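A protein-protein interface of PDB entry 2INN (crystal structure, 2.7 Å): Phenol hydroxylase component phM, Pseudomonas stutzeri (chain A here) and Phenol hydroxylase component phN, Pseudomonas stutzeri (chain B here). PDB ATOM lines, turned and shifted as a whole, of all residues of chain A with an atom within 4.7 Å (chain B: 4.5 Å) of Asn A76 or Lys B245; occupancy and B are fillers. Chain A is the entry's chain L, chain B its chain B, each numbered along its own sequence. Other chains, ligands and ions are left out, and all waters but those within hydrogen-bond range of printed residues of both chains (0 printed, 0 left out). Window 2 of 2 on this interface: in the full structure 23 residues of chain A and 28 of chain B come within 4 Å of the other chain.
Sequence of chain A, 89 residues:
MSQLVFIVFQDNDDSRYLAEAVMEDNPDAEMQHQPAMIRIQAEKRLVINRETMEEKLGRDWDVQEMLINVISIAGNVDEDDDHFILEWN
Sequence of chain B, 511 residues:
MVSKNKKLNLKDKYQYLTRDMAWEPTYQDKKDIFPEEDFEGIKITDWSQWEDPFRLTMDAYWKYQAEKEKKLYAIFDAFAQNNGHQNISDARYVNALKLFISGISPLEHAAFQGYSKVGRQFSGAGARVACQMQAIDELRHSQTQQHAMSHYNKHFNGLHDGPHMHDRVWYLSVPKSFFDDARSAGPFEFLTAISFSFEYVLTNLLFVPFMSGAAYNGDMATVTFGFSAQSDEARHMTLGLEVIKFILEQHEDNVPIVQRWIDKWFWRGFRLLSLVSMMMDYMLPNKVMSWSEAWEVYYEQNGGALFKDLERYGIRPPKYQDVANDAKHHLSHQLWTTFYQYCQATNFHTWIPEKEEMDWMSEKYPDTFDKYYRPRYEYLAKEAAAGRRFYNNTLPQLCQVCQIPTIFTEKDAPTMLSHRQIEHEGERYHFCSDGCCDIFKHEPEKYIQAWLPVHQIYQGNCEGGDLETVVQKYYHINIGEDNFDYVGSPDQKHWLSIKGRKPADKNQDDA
NZ of Lys B245 lies within hydrogen-bond range of OD1 of Asn A76 (3.3 Å).
The side-chain carboxylate (OD1) of Asp B309 lies within salt-bridge range of the side-chain amino group (NZ) of Lys B245 (3.1 Å).
The side-chain amino group (NZ) of Lys B245 sits close to the side-chain hydroxyl (OH) of Tyr B313.
NH2 of Arg B312 is in salt-bridge range of OD1 of Asp B309.
ND2 of Asn A76 sits at hydrogen-bond distance from O of Glu A87 (2.4 Å).
Among the printed residues, pairs that only touch across the chains: Asn A76 with Leu B241 and Trp A88 with Asp B309.
Asn A76 touches two residues of chain B.
Of the printed residues of chain B, Trp A88 touches Asp B309 (3.6 Å).
Of the printed residues of chain A, Leu B241 touches Asn A76 (3.2 Å).
Lys B245 touches one residue of chain A.
Phe B246 touches none of the printed residues of chain A.
Of the printed residues of chain A, Asp B309 touches Trp A88.
Of the 8 printed residues of chain A, 2 touch a printed residue of chain B.
Printed residues of chain A that touch a printed residue of chain B: Asn A76 and Trp A88.
Hydrophobic or aromatic side chains of chain A within 4 Å of the printed part of chain B: Trp A88.
Of the 12 printed residues of chain B, 3 touch a printed residue of chain A.
Printed residues of chain B that touch a printed residue of chain A: Leu B241, Lys B245 and Asp B309.
Along chain B the printed residues that touch a printed residue of chain A span positions 241 to 309.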
ATOM      1  N   GLY A  75     -30.432  -8.146 -27.669  1.00  0.00           N
ATOM      2  CA  GLY A  75     -28.992  -7.903 -27.908  1.00  0.00           C
ATOM      3  C   GLY A  75     -27.965  -8.691 -27.071  1.00  0.00           C
ATOM      4  O   GLY A  75     -28.315  -9.404 -26.093  1.00  0.00           O
ATOM      5  N   ASN A  76     -26.684  -8.582 -27.481  1.00  0.00           N
ATOM      6  CA  ASN A  76     -25.505  -9.157 -26.756  1.00  0.00           C
ATOM      7  C   ASN A  76     -25.178  -8.268 -25.562  1.00  0.00           C
ATOM      8  O   ASN A  76     -25.357  -7.049 -25.646  1.00  0.00           O
ATOM      9  CB  ASN A  76     -24.270  -9.236 -27.659  1.00  0.00           C
ATOM     10  CG  ASN A  76     -24.544  -9.955 -28.970  1.00  0.00           C
ATOM     11  OD1 ASN A  76     -24.285 -11.165 -29.086  1.00  0.00           O
ATOM     12  ND2 ASN A  76     -25.085  -9.220 -29.974  1.00  0.00           N
ATOM     13  N   VAL A  77     -24.682  -8.846 -24.469  1.00  0.00           N
ATOM     14  CA  VAL A  77     -24.613  -8.099 -23.214  1.00  0.00           C
ATOM     15  C   VAL A  77     -23.224  -7.584 -22.906  1.00  0.00           C
ATOM     16  O   VAL A  77     -22.256  -8.293 -23.069  1.00  0.00           O
ATOM     17  CB  VAL A  77     -25.211  -8.898 -22.003  1.00  0.00           C
ATOM     18  CG1 VAL A  77     -24.834  -8.293 -20.666  1.00  0.00           C
ATOM     19  CG2 VAL A  77     -26.715  -8.951 -22.109  1.00  0.00           C
ATOM     20  N   ASP A  78     -23.137  -6.324 -22.479  1.00  0.00           N
ATOM     21  CA  ASP A  78     -21.887  -5.803 -21.952  1.00  0.00           C
ATOM     22  C   ASP A  78     -22.113  -5.186 -20.560  1.00  0.00           C
ATOM     23  O   ASP A  78     -22.453  -3.995 -20.420  1.00  0.00           O
ATOM     24  CB  ASP A  78     -21.257  -4.821 -22.921  1.00  0.00           C
ATOM     25  CG  ASP A  78     -19.840  -4.498 -22.554  1.00  0.00           C
ATOM     26  OD1 ASP A  78     -19.602  -4.172 -21.357  1.00  0.00           O
ATOM     27  OD2 ASP A  78     -18.985  -4.558 -23.468  1.00  0.00           O
ATOM     28  N   ILE A  85     -24.315  -1.939 -21.907  1.00  0.00           N
ATOM     29  CA  ILE A  85     -24.379  -1.855 -23.362  1.00  0.00           C
ATOM     30  C   ILE A  85     -24.999  -3.127 -24.021  1.00  0.00           C
ATOM     31  O   ILE A  85     -24.610  -4.272 -23.750  1.00  0.00           O
ATOM     32  CB  ILE A  85     -22.990  -1.557 -24.005  1.00  0.00           C
ATOM     33  CG1 ILE A  85     -22.140  -0.600 -23.152  1.00  0.00           C
ATOM     34  CG2 ILE A  85     -23.187  -0.982 -25.404  1.00  0.00           C
ATOM     35  CD1 ILE A  85     -20.650  -0.591 -23.514  1.00  0.00           C
ATOM     36  N   LEU A  86     -25.955  -2.894 -24.910  1.00  0.00           N
ATOM     37  CA  LEU A  86     -26.769  -3.912 -25.536  1.00  0.00           C
ATOM     38  C   LEU A  86     -26.625  -3.679 -27.057  1.00  0.00           C
ATOM     39  O   LEU A  86     -26.951  -2.601 -27.554  1.00  0.00           O
ATOM     40  CB  LEU A  86     -28.231  -3.731 -25.072  1.00  0.00           C
ATOM     41  CG  LEU A  86     -28.946  -4.963 -24.489  1.00  0.00           C
ATOM     42  CD1 LEU A  86     -30.295  -4.664 -23.889  1.00  0.00           C
ATOM     43  CD2 LEU A  86     -29.098  -6.076 -25.496  1.00  0.00           C
ATOM     44  N   GLU A  87     -26.145  -4.682 -27.799  1.00  0.00           N
ATOM     45  CA  GLU A  87     -25.869  -4.461 -29.232  1.00  0.00           C
ATOM     46  C   GLU A  87     -25.563  -5.651 -30.166  1.00  0.00           C
ATOM     47  O   GLU A  87     -25.392  -6.818 -29.737  1.00  0.00           O
ATOM     48  CB  GLU A  87     -24.731  -3.461 -29.369  1.00  0.00           C
ATOM     49  CG  GLU A  87     -23.326  -3.996 -29.068  1.00  0.00           C
ATOM     50  CD  GLU A  87     -22.334  -2.855 -29.068  1.00  0.00           C
ATOM     51  OE1 GLU A  87     -21.586  -2.793 -28.072  1.00  0.00           O
ATOM     52  OE2 GLU A  87     -22.343  -2.002 -30.011  1.00  0.00           O
ATOM     53  N   TRP A  88     -25.479  -5.321 -31.453  1.00  0.00           N
ATOM     54  CA  TRP A  88     -25.006  -6.234 -32.461  1.00  0.00           C
ATOM     55  C   TRP A  88     -23.627  -5.740 -32.946  1.00  0.00           C
ATOM     56  O   TRP A  88     -23.376  -4.537 -32.929  1.00  0.00           O
ATOM     57  CB  TRP A  88     -26.038  -6.292 -33.585  1.00  0.00           C
ATOM     58  CG  TRP A  88     -27.509  -6.527 -33.102  1.00  0.00           C
ATOM     59  CD1 TRP A  88     -28.556  -5.621 -33.107  1.00  0.00           C
ATOM     60  CD2 TRP A  88     -28.061  -7.751 -32.558  1.00  0.00           C
ATOM     61  NE1 TRP A  88     -29.706  -6.214 -32.603  1.00  0.00           N
ATOM     62  CE2 TRP A  88     -29.422  -7.509 -32.261  1.00  0.00           C
ATOM     63  CE3 TRP A  88     -27.523  -9.034 -32.285  1.00  0.00           C
ATOM     64  CZ2 TRP A  88     -30.239  -8.494 -31.738  1.00  0.00           C
ATOM     65  CZ3 TRP A  88     -28.336  -9.994 -31.754  1.00  0.00           C
ATOM     66  CH2 TRP A  88     -29.674  -9.725 -31.485  1.00  0.00           C
ATOM     67  N   LEU B 241     -28.576 -16.741 -27.082  1.00  0.00           N
ATOM     68  CA  LEU B 241     -27.480 -16.008 -27.693  1.00  0.00           C
ATOM     69  C   LEU B 241     -26.093 -16.506 -27.273  1.00  0.00           C
ATOM     70  O   LEU B 241     -25.297 -17.008 -28.061  1.00  0.00           O
ATOM     71  CB  LEU B 241     -27.603 -14.556 -27.306  1.00  0.00           C
ATOM     72  CG  LEU B 241     -27.404 -13.524 -28.385  1.00  0.00           C
ATOM     73  CD1 LEU B 241     -26.086 -13.829 -28.999  1.00  0.00           C
ATOM     74  CD2 LEU B 241     -28.533 -13.565 -29.474  1.00  0.00           C
ATOM     75  N   GLU B 242     -25.751 -16.416 -26.024  1.00  0.00           N
ATOM     76  CA  GLU B 242     -24.321 -16.547 -25.837  1.00  0.00           C
ATOM     77  C   GLU B 242     -23.819 -17.936 -26.000  1.00  0.00           C
ATOM     78  O   GLU B 242     -22.620 -18.185 -25.989  1.00  0.00           O
ATOM     79  CB  GLU B 242     -23.817 -15.877 -24.551  1.00  0.00           C
ATOM     80  CG  GLU B 242     -23.278 -14.417 -24.831  1.00  0.00           C
ATOM     81  CD  GLU B 242     -21.846 -14.290 -24.332  1.00  0.00           C
ATOM     82  OE1 GLU B 242     -21.150 -15.352 -24.301  1.00  0.00           O
ATOM     83  OE2 GLU B 242     -21.422 -13.156 -23.971  1.00  0.00           O
ATOM     84  N   VAL B 243     -24.750 -18.851 -26.174  1.00  0.00           N
ATOM     85  CA  VAL B 243     -24.356 -20.240 -26.143  1.00  0.00           C
ATOM     86  C   VAL B 243     -24.324 -20.799 -27.513  1.00  0.00           C
ATOM     87  O   VAL B 243     -23.388 -21.461 -27.832  1.00  0.00           O
ATOM     88  CB  VAL B 243     -25.147 -21.114 -25.148  1.00  0.00           C
ATOM     89  CG1 VAL B 243     -26.509 -21.556 -25.748  1.00  0.00           C
ATOM     90  CG2 VAL B 243     -24.317 -22.312 -24.788  1.00  0.00           C
ATOM     91  N   ILE B 244     -25.276 -20.494 -28.362  1.00  0.00           N
ATOM     92  CA  ILE B 244     -24.945 -20.823 -29.718  1.00  0.00           C
ATOM     93  C   ILE B 244     -23.611 -20.122 -30.223  1.00  0.00           C
ATOM     94  O   ILE B 244     -22.709 -20.811 -30.798  1.00  0.00           O
ATOM     95  CB  ILE B 244     -26.104 -20.681 -30.687  1.00  0.00           C
ATOM     96  CG1 ILE B 244     -26.556 -19.238 -30.710  1.00  0.00           C
ATOM     97  CG2 ILE B 244     -27.192 -21.648 -30.322  1.00  0.00           C
ATOM     98  CD1 ILE B 244     -25.665 -18.306 -31.589  1.00  0.00           C
ATOM     99  N   LYS B 245     -23.442 -18.809 -29.976  1.00  0.00           N
ATOM    100  CA  LYS B 245     -22.207 -18.180 -30.418  1.00  0.00           C
ATOM    101  C   LYS B 245     -21.037 -19.020 -29.957  1.00  0.00           C
ATOM    102  O   LYS B 245     -19.984 -19.039 -30.578  1.00  0.00           O
ATOM    103  CB  LYS B 245     -22.018 -16.788 -29.847  1.00  0.00           C
ATOM    104  CG  LYS B 245     -22.845 -15.694 -30.478  1.00  0.00           C
ATOM    105  CD  LYS B 245     -22.795 -14.407 -29.567  1.00  0.00           C
ATOM    106  CE  LYS B 245     -21.831 -13.309 -30.078  1.00  0.00           C
ATOM    107  NZ  LYS B 245     -22.369 -12.681 -31.314  1.00  0.00           N
ATOM    108  N   PHE B 246     -21.204 -19.682 -28.829  1.00  0.00           N
ATOM    109  CA  PHE B 246     -20.072 -20.336 -28.205  1.00  0.00           C
ATOM    110  C   PHE B 246     -19.943 -21.675 -28.860  1.00  0.00           C
ATOM    111  O   PHE B 246     -18.887 -22.046 -29.308  1.00  0.00           O
ATOM    112  CB  PHE B 246     -20.287 -20.471 -26.699  1.00  0.00           C
ATOM    113  CG  PHE B 246     -19.403 -21.461 -26.071  1.00  0.00           C
ATOM    114  CD1 PHE B 246     -18.064 -21.176 -25.863  1.00  0.00           C
ATOM    115  CD2 PHE B 246     -19.896 -22.701 -25.691  1.00  0.00           C
ATOM    116  CE1 PHE B 246     -17.205 -22.144 -25.255  1.00  0.00           C
ATOM    117  CE2 PHE B 246     -19.072 -23.694 -25.091  1.00  0.00           C
ATOM    118  CZ  PHE B 246     -17.746 -23.424 -24.870  1.00  0.00           C
ATOM    119  N   ILE B 247     -21.043 -22.391 -28.931  1.00  0.00           N
ATOM    120  CA  ILE B 247     -21.083 -23.648 -29.630  1.00  0.00           C
ATOM    121  C   ILE B 247     -20.601 -23.513 -31.048  1.00  0.00           C
ATOM    122  O   ILE B 247     -19.902 -24.401 -31.527  1.00  0.00           O
ATOM    123  CB  ILE B 247     -22.521 -24.250 -29.690  1.00  0.00           C
ATOM    124  CG1 ILE B 247     -23.063 -24.664 -28.307  1.00  0.00           C
ATOM    125  CG2 ILE B 247     -22.556 -25.476 -30.619  1.00  0.00           C
ATOM    126  CD1 ILE B 247     -24.619 -24.916 -28.370  1.00  0.00           C
ATOM    127  N   LEU B 248     -20.988 -22.475 -31.760  1.00  0.00           N
ATOM    128  CA  LEU B 248     -20.680 -22.496 -33.176  1.00  0.00           C
ATOM    129  C   LEU B 248     -19.238 -22.270 -33.372  1.00  0.00           C
ATOM    130  O   LEU B 248     -18.619 -22.799 -34.281  1.00  0.00           O
ATOM    131  CB  LEU B 248     -21.401 -21.421 -33.930  1.00  0.00           C
ATOM    132  CG  LEU B 248     -22.924 -21.339 -33.948  1.00  0.00           C
ATOM    133  CD1 LEU B 248     -23.294 -19.905 -33.917  1.00  0.00           C
ATOM    134  CD2 LEU B 248     -23.485 -21.984 -35.179  1.00  0.00           C
ATOM    135  N   GLU B 249     -18.668 -21.457 -32.543  1.00  0.00           N
ATOM    136  CA  GLU B 249     -17.389 -21.014 -32.905  1.00  0.00           C
ATOM    137  C   GLU B 249     -16.457 -21.911 -32.166  1.00  0.00           C
ATOM    138  O   GLU B 249     -15.279 -21.646 -32.085  1.00  0.00           O
ATOM    139  CB  GLU B 249     -17.203 -19.504 -32.621  1.00  0.00           C
ATOM    140  CG  GLU B 249     -16.503 -19.107 -31.323  1.00  0.00           C
ATOM    141  CD  GLU B 249     -16.463 -17.535 -31.077  1.00  0.00           C
ATOM    142  OE1 GLU B 249     -17.441 -16.945 -30.516  1.00  0.00           O
ATOM    143  OE2 GLU B 249     -15.437 -16.898 -31.441  1.00  0.00           O
ATOM    144  N   ASP B 309     -26.494 -10.987 -37.426  1.00  0.00           N
ATOM    145  CA  ASP B 309     -25.351 -11.152 -36.505  1.00  0.00           C
ATOM    146  C   ASP B 309     -24.807 -12.599 -36.424  1.00  0.00           C
ATOM    147  O   ASP B 309     -23.866 -12.863 -35.647  1.00  0.00           O
ATOM    148  CB  ASP B 309     -25.657 -10.602 -35.088  1.00  0.00           C
ATOM    149  CG  ASP B 309     -24.346 -10.264 -34.257  1.00  0.00           C
ATOM    150  OD1 ASP B 309     -23.891 -11.229 -33.540  1.00  0.00           O
ATOM    151  OD2 ASP B 309     -23.800  -9.071 -34.340  1.00  0.00           O
ATOM    152  N   ARG B 312     -21.976 -14.216 -39.903  1.00  0.00           N
ATOM    153  CA  ARG B 312     -20.614 -14.254 -39.499  1.00  0.00           C
ATOM    154  C   ARG B 312     -20.139 -15.633 -39.060  1.00  0.00           C
ATOM    155  O   ARG B 312     -19.004 -15.959 -39.330  1.00  0.00           O
ATOM    156  CB  ARG B 312     -20.406 -13.202 -38.465  1.00  0.00           C
ATOM    157  CG  ARG B 312     -21.047 -11.878 -39.026  1.00  0.00           C
ATOM    158  CD  ARG B 312     -20.696 -10.547 -38.235  1.00  0.00           C
ATOM    159  NE  ARG B 312     -21.127 -10.565 -36.818  1.00  0.00           N
ATOM    160  CZ  ARG B 312     -20.681 -11.425 -35.900  1.00  0.00           C
ATOM    161  NH1 ARG B 312     -19.796 -12.387 -36.217  1.00  0.00           N
ATOM    162  NH2 ARG B 312     -21.139 -11.339 -34.664  1.00  0.00           N
ATOM    163  N   TYR B 313     -20.991 -16.467 -38.438  1.00  0.00           N
ATOM    164  CA  TYR B 313     -20.567 -17.855 -37.976  1.00  0.00           C
ATOM    165  C   TYR B 313     -20.869 -18.997 -38.971  1.00  0.00           C
ATOM    166  O   TYR B 313     -20.593 -20.190 -38.677  1.00  0.00           O
ATOM    167  CB  TYR B 313     -21.108 -18.268 -36.592  1.00  0.00           C
ATOM    168  CG  TYR B 313     -20.802 -17.333 -35.457  1.00  0.00           C
ATOM    169  CD1 TYR B 313     -21.591 -16.198 -35.258  1.00  0.00           C
ATOM    170  CD2 TYR B 313     -19.711 -17.562 -34.560  1.00  0.00           C
ATOM    171  CE1 TYR B 313     -21.307 -15.263 -34.204  1.00  0.00           C
ATOM    172  CE2 TYR B 313     -19.410 -16.629 -33.464  1.00  0.00           C
ATOM    173  CZ  TYR B 313     -20.241 -15.487 -33.303  1.00  0.00           C
ATOM    174  OH  TYR B 313     -20.087 -14.543 -32.296  1.00  0.00           O
